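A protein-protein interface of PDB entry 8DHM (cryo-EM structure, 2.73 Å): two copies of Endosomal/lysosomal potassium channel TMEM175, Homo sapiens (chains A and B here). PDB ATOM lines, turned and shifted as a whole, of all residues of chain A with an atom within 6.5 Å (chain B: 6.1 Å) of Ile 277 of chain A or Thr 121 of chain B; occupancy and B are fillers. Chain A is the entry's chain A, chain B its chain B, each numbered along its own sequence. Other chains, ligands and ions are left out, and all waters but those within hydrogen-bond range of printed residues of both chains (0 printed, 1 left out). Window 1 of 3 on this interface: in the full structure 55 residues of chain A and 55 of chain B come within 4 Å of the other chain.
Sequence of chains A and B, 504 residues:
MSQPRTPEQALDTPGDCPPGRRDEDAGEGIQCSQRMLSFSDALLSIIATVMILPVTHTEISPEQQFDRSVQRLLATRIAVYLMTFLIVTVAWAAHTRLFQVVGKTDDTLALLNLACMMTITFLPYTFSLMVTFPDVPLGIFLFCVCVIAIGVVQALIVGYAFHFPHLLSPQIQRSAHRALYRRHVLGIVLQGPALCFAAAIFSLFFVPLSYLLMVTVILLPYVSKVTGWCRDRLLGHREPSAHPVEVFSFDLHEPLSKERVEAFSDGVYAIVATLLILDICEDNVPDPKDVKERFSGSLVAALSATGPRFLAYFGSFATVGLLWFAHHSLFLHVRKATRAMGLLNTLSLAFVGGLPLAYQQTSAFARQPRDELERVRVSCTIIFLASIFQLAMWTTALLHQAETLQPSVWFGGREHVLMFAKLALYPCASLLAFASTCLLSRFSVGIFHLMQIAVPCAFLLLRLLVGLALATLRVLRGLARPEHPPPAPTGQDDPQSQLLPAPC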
ATOM      1  N   ALA A 273      30.660   6.789  -7.881  1.00  0.00           N
ATOM      2  CA  ALA A 273      30.037   5.914  -8.866  1.00  0.00           C
ATOM      3  C   ALA A 273      29.241   6.684  -9.913  1.00  0.00           C
ATOM      4  O   ALA A 273      29.235   6.291 -11.084  1.00  0.00           O
ATOM      5  CB  ALA A 273      29.138   4.905  -8.162  1.00  0.00           C
ATOM      6  N   THR A 274      28.554   7.760  -9.526  1.00  0.00           N
ATOM      7  CA  THR A 274      27.706   8.496 -10.464  1.00  0.00           C
ATOM      8  C   THR A 274      28.377   9.741 -11.042  1.00  0.00           C
ATOM      9  O   THR A 274      27.739  10.494 -11.801  1.00  0.00           O
ATOM     10  CB  THR A 274      26.391   8.870  -9.784  1.00  0.00           C
ATOM     11  OG1 THR A 274      26.658   9.521  -8.539  1.00  0.00           O
ATOM     12  CG2 THR A 274      25.579   7.635  -9.530  1.00  0.00           C
ATOM     13  N   LEU A 275      29.644   9.976 -10.698  1.00  0.00           N
ATOM     14  CA  LEU A 275      30.351  11.160 -11.177  1.00  0.00           C
ATOM     15  C   LEU A 275      30.273  11.305 -12.692  1.00  0.00           C
ATOM     16  O   LEU A 275      29.962  12.388 -13.200  1.00  0.00           O
ATOM     17  CB  LEU A 275      31.806  11.091 -10.731  1.00  0.00           C
ATOM     18  CG  LEU A 275      32.530  12.405 -10.482  1.00  0.00           C
ATOM     19  CD1 LEU A 275      32.030  13.042  -9.212  1.00  0.00           C
ATOM     20  CD2 LEU A 275      34.001  12.143 -10.393  1.00  0.00           C
ATOM     21  N   LEU A 276      30.569  10.242 -13.432  1.00  0.00           N
ATOM     22  CA  LEU A 276      30.662  10.343 -14.882  1.00  0.00           C
ATOM     23  C   LEU A 276      29.306  10.412 -15.561  1.00  0.00           C
ATOM     24  O   LEU A 276      29.171  11.080 -16.594  1.00  0.00           O
ATOM     25  CB  LEU A 276      31.458   9.161 -15.440  1.00  0.00           C
ATOM     26  CG  LEU A 276      32.929   9.070 -15.038  1.00  0.00           C
ATOM     27  CD1 LEU A 276      33.622   8.065 -15.909  1.00  0.00           C
ATOM     28  CD2 LEU A 276      33.637  10.413 -15.118  1.00  0.00           C
ATOM     29  N   ILE A 277      28.292   9.744 -15.013  1.00  0.00           N
ATOM     30  CA  ILE A 277      26.962   9.871 -15.587  1.00  0.00           C
ATOM     31  C   ILE A 277      26.432  11.284 -15.398  1.00  0.00           C
ATOM     32  O   ILE A 277      25.681  11.788 -16.243  1.00  0.00           O
ATOM     33  CB  ILE A 277      26.009   8.814 -15.001  1.00  0.00           C
ATOM     34  CG1 ILE A 277      24.732   8.735 -15.831  1.00  0.00           C
ATOM     35  CG2 ILE A 277      25.689   9.091 -13.547  1.00  0.00           C
ATOM     36  CD1 ILE A 277      24.880   7.946 -17.081  1.00  0.00           C
ATOM     37  N   LEU A 278      26.805  11.954 -14.305  1.00  0.00           N
ATOM     38  CA  LEU A 278      26.397  13.350 -14.163  1.00  0.00           C
ATOM     39  C   LEU A 278      26.929  14.203 -15.312  1.00  0.00           C
ATOM     40  O   LEU A 278      26.187  15.001 -15.900  1.00  0.00           O
ATOM     41  CB  LEU A 278      26.868  13.914 -12.827  1.00  0.00           C
ATOM     42  CG  LEU A 278      26.213  13.377 -11.555  1.00  0.00           C
ATOM     43  CD1 LEU A 278      26.871  14.000 -10.355  1.00  0.00           C
ATOM     44  CD2 LEU A 278      24.729  13.629 -11.530  1.00  0.00           C
ATOM     45  N   ASP A 279      28.210  14.046 -15.648  1.00  0.00           N
ATOM     46  CA  ASP A 279      28.781  14.785 -16.767  1.00  0.00           C
ATOM     47  C   ASP A 279      28.142  14.391 -18.089  1.00  0.00           C
ATOM     48  O   ASP A 279      27.909  15.251 -18.944  1.00  0.00           O
ATOM     49  CB  ASP A 279      30.285  14.555 -16.830  1.00  0.00           C
ATOM     50  CG  ASP A 279      31.050  15.517 -15.961  1.00  0.00           C
ATOM     51  OD1 ASP A 279      31.855  15.054 -15.125  1.00  0.00           O
ATOM     52  OD2 ASP A 279      30.845  16.740 -16.113  1.00  0.00           O
ATOM     53  N   ILE A 280      27.868  13.101 -18.281  1.00  0.00           N
ATOM     54  CA  ILE A 280      27.223  12.673 -19.515  1.00  0.00           C
ATOM     55  C   ILE A 280      25.867  13.345 -19.665  1.00  0.00           C
ATOM     56  O   ILE A 280      25.515  13.811 -20.756  1.00  0.00           O
ATOM     57  CB  ILE A 280      27.102  11.141 -19.545  1.00  0.00           C
ATOM     58  CG1 ILE A 280      28.468  10.516 -19.819  1.00  0.00           C
ATOM     59  CG2 ILE A 280      26.094  10.714 -20.591  1.00  0.00           C
ATOM     60  CD1 ILE A 280      28.561   9.075 -19.443  1.00  0.00           C
ATOM     61  N   CYS A 281      25.085  13.406 -18.590  1.00  0.00           N
ATOM     62  CA  CYS A 281      23.799  14.088 -18.630  1.00  0.00           C
ATOM     63  C   CYS A 281      23.932  15.586 -18.873  1.00  0.00           C
ATOM     64  O   CYS A 281      23.116  16.152 -19.607  1.00  0.00           O
ATOM     65  CB  CYS A 281      23.038  13.845 -17.329  1.00  0.00           C
ATOM     66  SG  CYS A 281      22.356  12.187 -17.148  1.00  0.00           S
ATOM     67  N   GLU A 282      24.929  16.239 -18.276  1.00  0.00           N
ATOM     68  CA  GLU A 282      25.102  17.677 -18.450  1.00  0.00           C
ATOM     69  C   GLU A 282      25.619  18.087 -19.824  1.00  0.00           C
ATOM     70  O   GLU A 282      25.190  19.125 -20.340  1.00  0.00           O
ATOM     71  CB  GLU A 282      26.072  18.232 -17.408  1.00  0.00           C
ATOM     72  CG  GLU A 282      25.579  18.193 -15.975  1.00  0.00           C
ATOM     73  CD  GLU A 282      26.606  18.740 -15.005  1.00  0.00           C
ATOM     74  OE1 GLU A 282      27.740  19.028 -15.441  1.00  0.00           O
ATOM     75  OE2 GLU A 282      26.284  18.889 -13.811  1.00  0.00           O
ATOM     76  N   PHE A 310      30.415   6.507 -22.180  1.00  0.00           N
ATOM     77  CA  PHE A 310      29.526   5.511 -21.595  1.00  0.00           C
ATOM     78  C   PHE A 310      30.300   4.291 -21.112  1.00  0.00           C
ATOM     79  O   PHE A 310      29.997   3.743 -20.049  1.00  0.00           O
ATOM     80  CB  PHE A 310      28.467   5.104 -22.613  1.00  0.00           C
ATOM     81  CG  PHE A 310      27.405   6.133 -22.825  1.00  0.00           C
ATOM     82  CD1 PHE A 310      26.491   6.420 -21.830  1.00  0.00           C
ATOM     83  CD2 PHE A 310      27.314   6.809 -24.025  1.00  0.00           C
ATOM     84  CE1 PHE A 310      25.513   7.366 -22.029  1.00  0.00           C
ATOM     85  CE2 PHE A 310      26.338   7.752 -24.225  1.00  0.00           C
ATOM     86  CZ  PHE A 310      25.437   8.031 -23.227  1.00  0.00           C
ATOM     87  N   TYR A 313      31.935   5.229 -17.864  1.00  0.00           N
ATOM     88  CA  TYR A 313      30.985   5.235 -16.759  1.00  0.00           C
ATOM     89  C   TYR A 313      30.613   3.819 -16.340  1.00  0.00           C
ATOM     90  O   TYR A 313      30.538   3.523 -15.145  1.00  0.00           O
ATOM     91  CB  TYR A 313      29.734   6.021 -17.133  1.00  0.00           C
ATOM     92  CG  TYR A 313      28.573   5.714 -16.224  1.00  0.00           C
ATOM     93  CD1 TYR A 313      28.623   6.046 -14.882  1.00  0.00           C
ATOM     94  CD2 TYR A 313      27.437   5.079 -16.698  1.00  0.00           C
ATOM     95  CE1 TYR A 313      27.585   5.763 -14.043  1.00  0.00           C
ATOM     96  CE2 TYR A 313      26.391   4.793 -15.862  1.00  0.00           C
ATOM     97  CZ  TYR A 313      26.470   5.140 -14.532  1.00  0.00           C
ATOM     98  OH  TYR A 313      25.434   4.862 -13.680  1.00  0.00           O
ATOM     99  N   PHE A 317      31.471   2.676 -12.563  1.00  0.00           N
ATOM    100  CA  PHE A 317      30.365   2.333 -11.682  1.00  0.00           C
ATOM    101  C   PHE A 317      30.477   0.895 -11.203  1.00  0.00           C
ATOM    102  O   PHE A 317      30.284   0.617 -10.015  1.00  0.00           O
ATOM    103  CB  PHE A 317      29.038   2.563 -12.403  1.00  0.00           C
ATOM    104  CG  PHE A 317      27.825   2.290 -11.561  1.00  0.00           C
ATOM    105  CD1 PHE A 317      27.405   0.996 -11.313  1.00  0.00           C
ATOM    106  CD2 PHE A 317      27.102   3.330 -11.019  1.00  0.00           C
ATOM    107  CE1 PHE A 317      26.298   0.754 -10.543  1.00  0.00           C
ATOM    108  CE2 PHE A 317      25.994   3.090 -10.250  1.00  0.00           C
ATOM    109  CZ  PHE A 317      25.591   1.802 -10.010  1.00  0.00           C
ATOM    110  N   LEU B  43      22.132   6.846  -4.048  1.00  0.00           N
ATOM    111  CA  LEU B  43      22.252   6.841  -5.500  1.00  0.00           C
ATOM    112  C   LEU B  43      21.007   7.423  -6.155  1.00  0.00           C
ATOM    113  O   LEU B  43      21.101   8.242  -7.078  1.00  0.00           O
ATOM    114  CB  LEU B  43      22.502   5.418  -6.000  1.00  0.00           C
ATOM    115  CG  LEU B  43      23.876   4.828  -5.707  1.00  0.00           C
ATOM    116  CD1 LEU B  43      23.847   3.335  -5.876  1.00  0.00           C
ATOM    117  CD2 LEU B  43      24.918   5.436  -6.608  1.00  0.00           C
ATOM    118  N   ILE B  47      20.567  10.645  -8.706  1.00  0.00           N
ATOM    119  CA  ILE B  47      20.001  10.508 -10.041  1.00  0.00           C
ATOM    120  C   ILE B  47      18.753  11.367 -10.214  1.00  0.00           C
ATOM    121  O   ILE B  47      18.521  11.912 -11.298  1.00  0.00           O
ATOM    122  CB  ILE B  47      19.723   9.025 -10.330  1.00  0.00           C
ATOM    123  CG1 ILE B  47      21.023   8.222 -10.254  1.00  0.00           C
ATOM    124  CG2 ILE B  47      19.073   8.852 -11.680  1.00  0.00           C
ATOM    125  CD1 ILE B  47      22.152   8.769 -11.079  1.00  0.00           C
ATOM    126  N   VAL B  50      20.078  15.036 -10.708  1.00  0.00           N
ATOM    127  CA  VAL B  50      21.057  15.351 -11.751  1.00  0.00           C
ATOM    128  C   VAL B  50      20.605  16.537 -12.604  1.00  0.00           C
ATOM    129  O   VAL B  50      21.399  17.440 -12.893  1.00  0.00           O
ATOM    130  CB  VAL B  50      21.335  14.109 -12.619  1.00  0.00           C
ATOM    131  CG1 VAL B  50      20.093  13.658 -13.333  1.00  0.00           C
ATOM    132  CG2 VAL B  50      22.428  14.402 -13.633  1.00  0.00           C
ATOM    133  N   CYS B 116      20.379  -3.024 -10.760  1.00  0.00           N
ATOM    134  CA  CYS B 116      19.155  -2.236 -10.878  1.00  0.00           C
ATOM    135  C   CYS B 116      19.433  -0.745 -10.724  1.00  0.00           C
ATOM    136  O   CYS B 116      18.851   0.080 -11.439  1.00  0.00           O
ATOM    137  CB  CYS B 116      18.134  -2.700  -9.842  1.00  0.00           C
ATOM    138  SG  CYS B 116      16.734  -1.581  -9.640  1.00  0.00           S
ATOM    139  N   MET B 117      20.302  -0.377  -9.781  1.00  0.00           N
ATOM    140  CA  MET B 117      20.702   1.020  -9.649  1.00  0.00           C
ATOM    141  C   MET B 117      21.373   1.523 -10.917  1.00  0.00           C
ATOM    142  O   MET B 117      21.101   2.642 -11.370  1.00  0.00           O
ATOM    143  CB  MET B 117      21.641   1.193  -8.454  1.00  0.00           C
ATOM    144  CG  MET B 117      20.997   1.024  -7.089  1.00  0.00           C
ATOM    145  SD  MET B 117      19.633   2.149  -6.765  1.00  0.00           S
ATOM    146  CE  MET B 117      18.251   1.063  -7.078  1.00  0.00           C
ATOM    147  N   MET B 118      22.263   0.718 -11.498  1.00  0.00           N
ATOM    148  CA  MET B 118      22.880   1.092 -12.764  1.00  0.00           C
ATOM    149  C   MET B 118      21.820   1.392 -13.814  1.00  0.00           C
ATOM    150  O   MET B 118      21.883   2.417 -14.501  1.00  0.00           O
ATOM    151  CB  MET B 118      23.811  -0.024 -13.238  1.00  0.00           C
ATOM    152  CG  MET B 118      24.371   0.171 -14.639  1.00  0.00           C
ATOM    153  SD  MET B 118      25.395   1.640 -14.789  1.00  0.00           S
ATOM    154  CE  MET B 118      27.015   0.897 -14.775  1.00  0.00           C
ATOM    155  N   THR B 119      20.833   0.505 -13.950  1.00  0.00           N
ATOM    156  CA  THR B 119      19.788   0.732 -14.944  1.00  0.00           C
ATOM    157  C   THR B 119      18.993   2.000 -14.652  1.00  0.00           C
ATOM    158  O   THR B 119      18.696   2.768 -15.575  1.00  0.00           O
ATOM    159  CB  THR B 119      18.845  -0.470 -15.024  1.00  0.00           C
ATOM    160  OG1 THR B 119      18.203  -0.673 -13.761  1.00  0.00           O
ATOM    161  CG2 THR B 119      19.588  -1.717 -15.422  1.00  0.00           C
ATOM    162  N   ILE B 120      18.635   2.238 -13.390  1.00  0.00           N
ATOM    163  CA  ILE B 120      17.882   3.444 -13.058  1.00  0.00           C
ATOM    164  C   ILE B 120      18.692   4.691 -13.372  1.00  0.00           C
ATOM    165  O   ILE B 120      18.129   5.732 -13.721  1.00  0.00           O
ATOM    166  CB  ILE B 120      17.448   3.430 -11.583  1.00  0.00           C
ATOM    167  CG1 ILE B 120      16.381   2.361 -11.354  1.00  0.00           C
ATOM    168  CG2 ILE B 120      16.938   4.805 -11.166  1.00  0.00           C
ATOM    169  CD1 ILE B 120      16.119   2.061  -9.911  1.00  0.00           C
ATOM    170  N   THR B 121      20.011   4.610 -13.260  1.00  0.00           N
ATOM    171  CA  THR B 121      20.875   5.760 -13.478  1.00  0.00           C
ATOM    172  C   THR B 121      20.829   6.297 -14.907  1.00  0.00           C
ATOM    173  O   THR B 121      21.287   7.422 -15.134  1.00  0.00           O
ATOM    174  CB  THR B 121      22.303   5.382 -13.099  1.00  0.00           C
ATOM    175  OG1 THR B 121      22.353   5.034 -11.711  1.00  0.00           O
ATOM    176  CG2 THR B 121      23.230   6.509 -13.344  1.00  0.00           C
ATOM    177  N   PHE B 122      20.289   5.552 -15.868  1.00  0.00           N
ATOM    178  CA  PHE B 122      20.244   5.995 -17.254  1.00  0.00           C
ATOM    179  C   PHE B 122      18.938   6.676 -17.640  1.00  0.00           C
ATOM    180  O   PHE B 122      18.830   7.166 -18.769  1.00  0.00           O
ATOM    181  CB  PHE B 122      20.480   4.805 -18.197  1.00  0.00           C
ATOM    182  CG  PHE B 122      21.921   4.562 -18.518  1.00  0.00           C
ATOM    183  CD1 PHE B 122      22.675   5.523 -19.162  1.00  0.00           C
ATOM    184  CD2 PHE B 122      22.525   3.368 -18.174  1.00  0.00           C
ATOM    185  CE1 PHE B 122      23.998   5.298 -19.454  1.00  0.00           C
ATOM    186  CE2 PHE B 122      23.851   3.139 -18.465  1.00  0.00           C
ATOM    187  CZ  PHE B 122      24.586   4.105 -19.106  1.00  0.00           C
ATOM    188  N   LEU B 123      17.954   6.726 -16.748  1.00  0.00           N
ATOM    189  CA  LEU B 123      16.638   7.266 -17.061  1.00  0.00           C
ATOM    190  C   LEU B 123      16.695   8.745 -17.434  1.00  0.00           C
ATOM    191  O   LEU B 123      16.076   9.153 -18.425  1.00  0.00           O
ATOM    192  CB  LEU B 123      15.692   7.061 -15.881  1.00  0.00           C
ATOM    193  CG  LEU B 123      15.028   5.694 -15.752  1.00  0.00           C
ATOM    194  CD1 LEU B 123      14.416   5.575 -14.380  1.00  0.00           C
ATOM    195  CD2 LEU B 123      13.988   5.470 -16.823  1.00  0.00           C
ATOM    196  N   PRO B 124      17.391   9.585 -16.661  1.00  0.00           N
ATOM    197  CA  PRO B 124      17.437  11.012 -17.017  1.00  0.00           C
ATOM    198  C   PRO B 124      18.020  11.278 -18.389  1.00  0.00           C
ATOM    199  O   PRO B 124      17.476  12.095 -19.141  1.00  0.00           O
ATOM    200  CB  PRO B 124      18.301  11.615 -15.901  1.00  0.00           C
ATOM    201  CG  PRO B 124      18.222  10.662 -14.801  1.00  0.00           C
ATOM    202  CD  PRO B 124      18.096   9.324 -15.396  1.00  0.00           C
ATOM    203  N   TYR B 125      19.117  10.604 -18.739  1.00  0.00           N
ATOM    204  CA  TYR B 125      19.735  10.827 -20.039  1.00  0.00           C
ATOM    205  C   TYR B 125      18.799  10.435 -21.172  1.00  0.00           C
ATOM    206  O   TYR B 125      18.643  11.180 -22.144  1.00  0.00           O
ATOM    207  CB  TYR B 125      21.047  10.050 -20.129  1.00  0.00           C
ATOM    208  CG  TYR B 125      21.741  10.179 -21.461  1.00  0.00           C
ATOM    209  CD1 TYR B 125      21.500   9.277 -22.484  1.00  0.00           C
ATOM    210  CD2 TYR B 125      22.627  11.212 -21.701  1.00  0.00           C
ATOM    211  CE1 TYR B 125      22.123   9.396 -23.693  1.00  0.00           C
ATOM    212  CE2 TYR B 125      23.254  11.338 -22.908  1.00  0.00           C
ATOM    213  CZ  TYR B 125      23.000  10.430 -23.903  1.00  0.00           C
ATOM    214  OH  TYR B 125      23.630  10.558 -25.112  1.00  0.00           O
ATOM    215  N   CYS B 146      15.377   1.259 -21.135  1.00  0.00           N
ATOM    216  CA  CYS B 146      15.778   1.492 -19.750  1.00  0.00           C
ATOM    217  C   CYS B 146      14.704   1.013 -18.777  1.00  0.00           C
ATOM    218  O   CYS B 146      15.000   0.290 -17.811  1.00  0.00           O
ATOM    219  CB  CYS B 146      16.072   2.976 -19.537  1.00  0.00           C
ATOM    220  SG  CYS B 146      16.826   3.386 -17.950  1.00  0.00           S
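No position is printed for both chains.
Ile 277 of chain A touches two residues of chain B. Of the printed residues of chain B, Phe 317 of chain A touches Met 118 (3.5 Å). Printed residues of chain A within 4 Å of Ile 47 of chain B: Thr 274 (3.9 Å). Printed residues of chain A within 4 Å of Val 50 of chain B: Leu 278 (3.2 Å) and Cys 281 (3.8 Å). The nearest residue of chain B that does not touch Ile 277 of chain A is Ile 47 of chain B (4.3 Å). The nearest residue of chain A that does not touch Thr 121 of chain B is Phe 317 of chain A (4.4 Å). The nearest printed residue of chain B that does not touch Leu 278 of chain A is Ile 47 of chain B (5.5 Å).
Thr 274 of chain A touches Leu 43 of chain B (CG2 to CD2, 3.7 Å). Thr 274 of chain A touches Ile 47 of chain B (CG2 to CD1, 3.9 Å). CG2 of Ile 277 of chain A touches CG2 of Thr 121 of chain B (3.6 Å). Ile 277 of chain A touches Phe 122 of chain B (CD1 to CE1, 3.7 Å). Ile 280 of chain A touches Tyr 125 of chain B (CG2 to CD2, 3.7 Å). Val 50 of chain B touches Cys 281 of chain A. CZ of Tyr 125 of chain B touches CZ of Phe 310 of chain A, 3.5 Å away. CG2 of Thr 121 of chain B touches OH of Tyr 313 of chain A, 2.8 Å away. CZ of Phe 122 of chain B touches CE2 of Tyr 313 of chain A (3.8 Å). Phe 317 of chain A touches Met 118 of chain B (CD1 to CE, 3.5 Å).
The side-chain hydroxyl of Tyr 313 of chain A lies within hydrogen-bond range of the side-chain sulfur of Met 118 of chain B (3.4 Å).
Printed residues of chain A that touch a printed residue of chain B: Thr 274, Ile 277, Leu 278, Ile 280, Cys 281, Phe 310, Tyr 313 and Phe 317. Hydrophobic or aromatic side chains of chain A that line the printed part of chain B: Ile 277, Leu 278, Ile 280, Phe 310, Tyr 313 and Phe 317. Hydrophobic or aromatic side chains of chain B within 4 Å of the printed part of chain A: Leu 43, Ile 47, Val 50, Met 118, Phe 122 and Tyr 125. Among the printed residues, 14 pairs touch across the chains. Among the printed residues, no Asp or Glu carboxylate lies within 4 Å of a Lys or Arg side-chain nitrogen of the other chain.
The backbone carbonyl oxygen (O) of Met 117 of chain B lies within hydrogen-bond range of the side-chain hydroxyl (OG1) of Thr 121 of chain B (2.7 Å). SG of Cys 281 of chain A lies within hydrogen-bond range of O of Ile 277 of chain A, 3.5 Å away.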
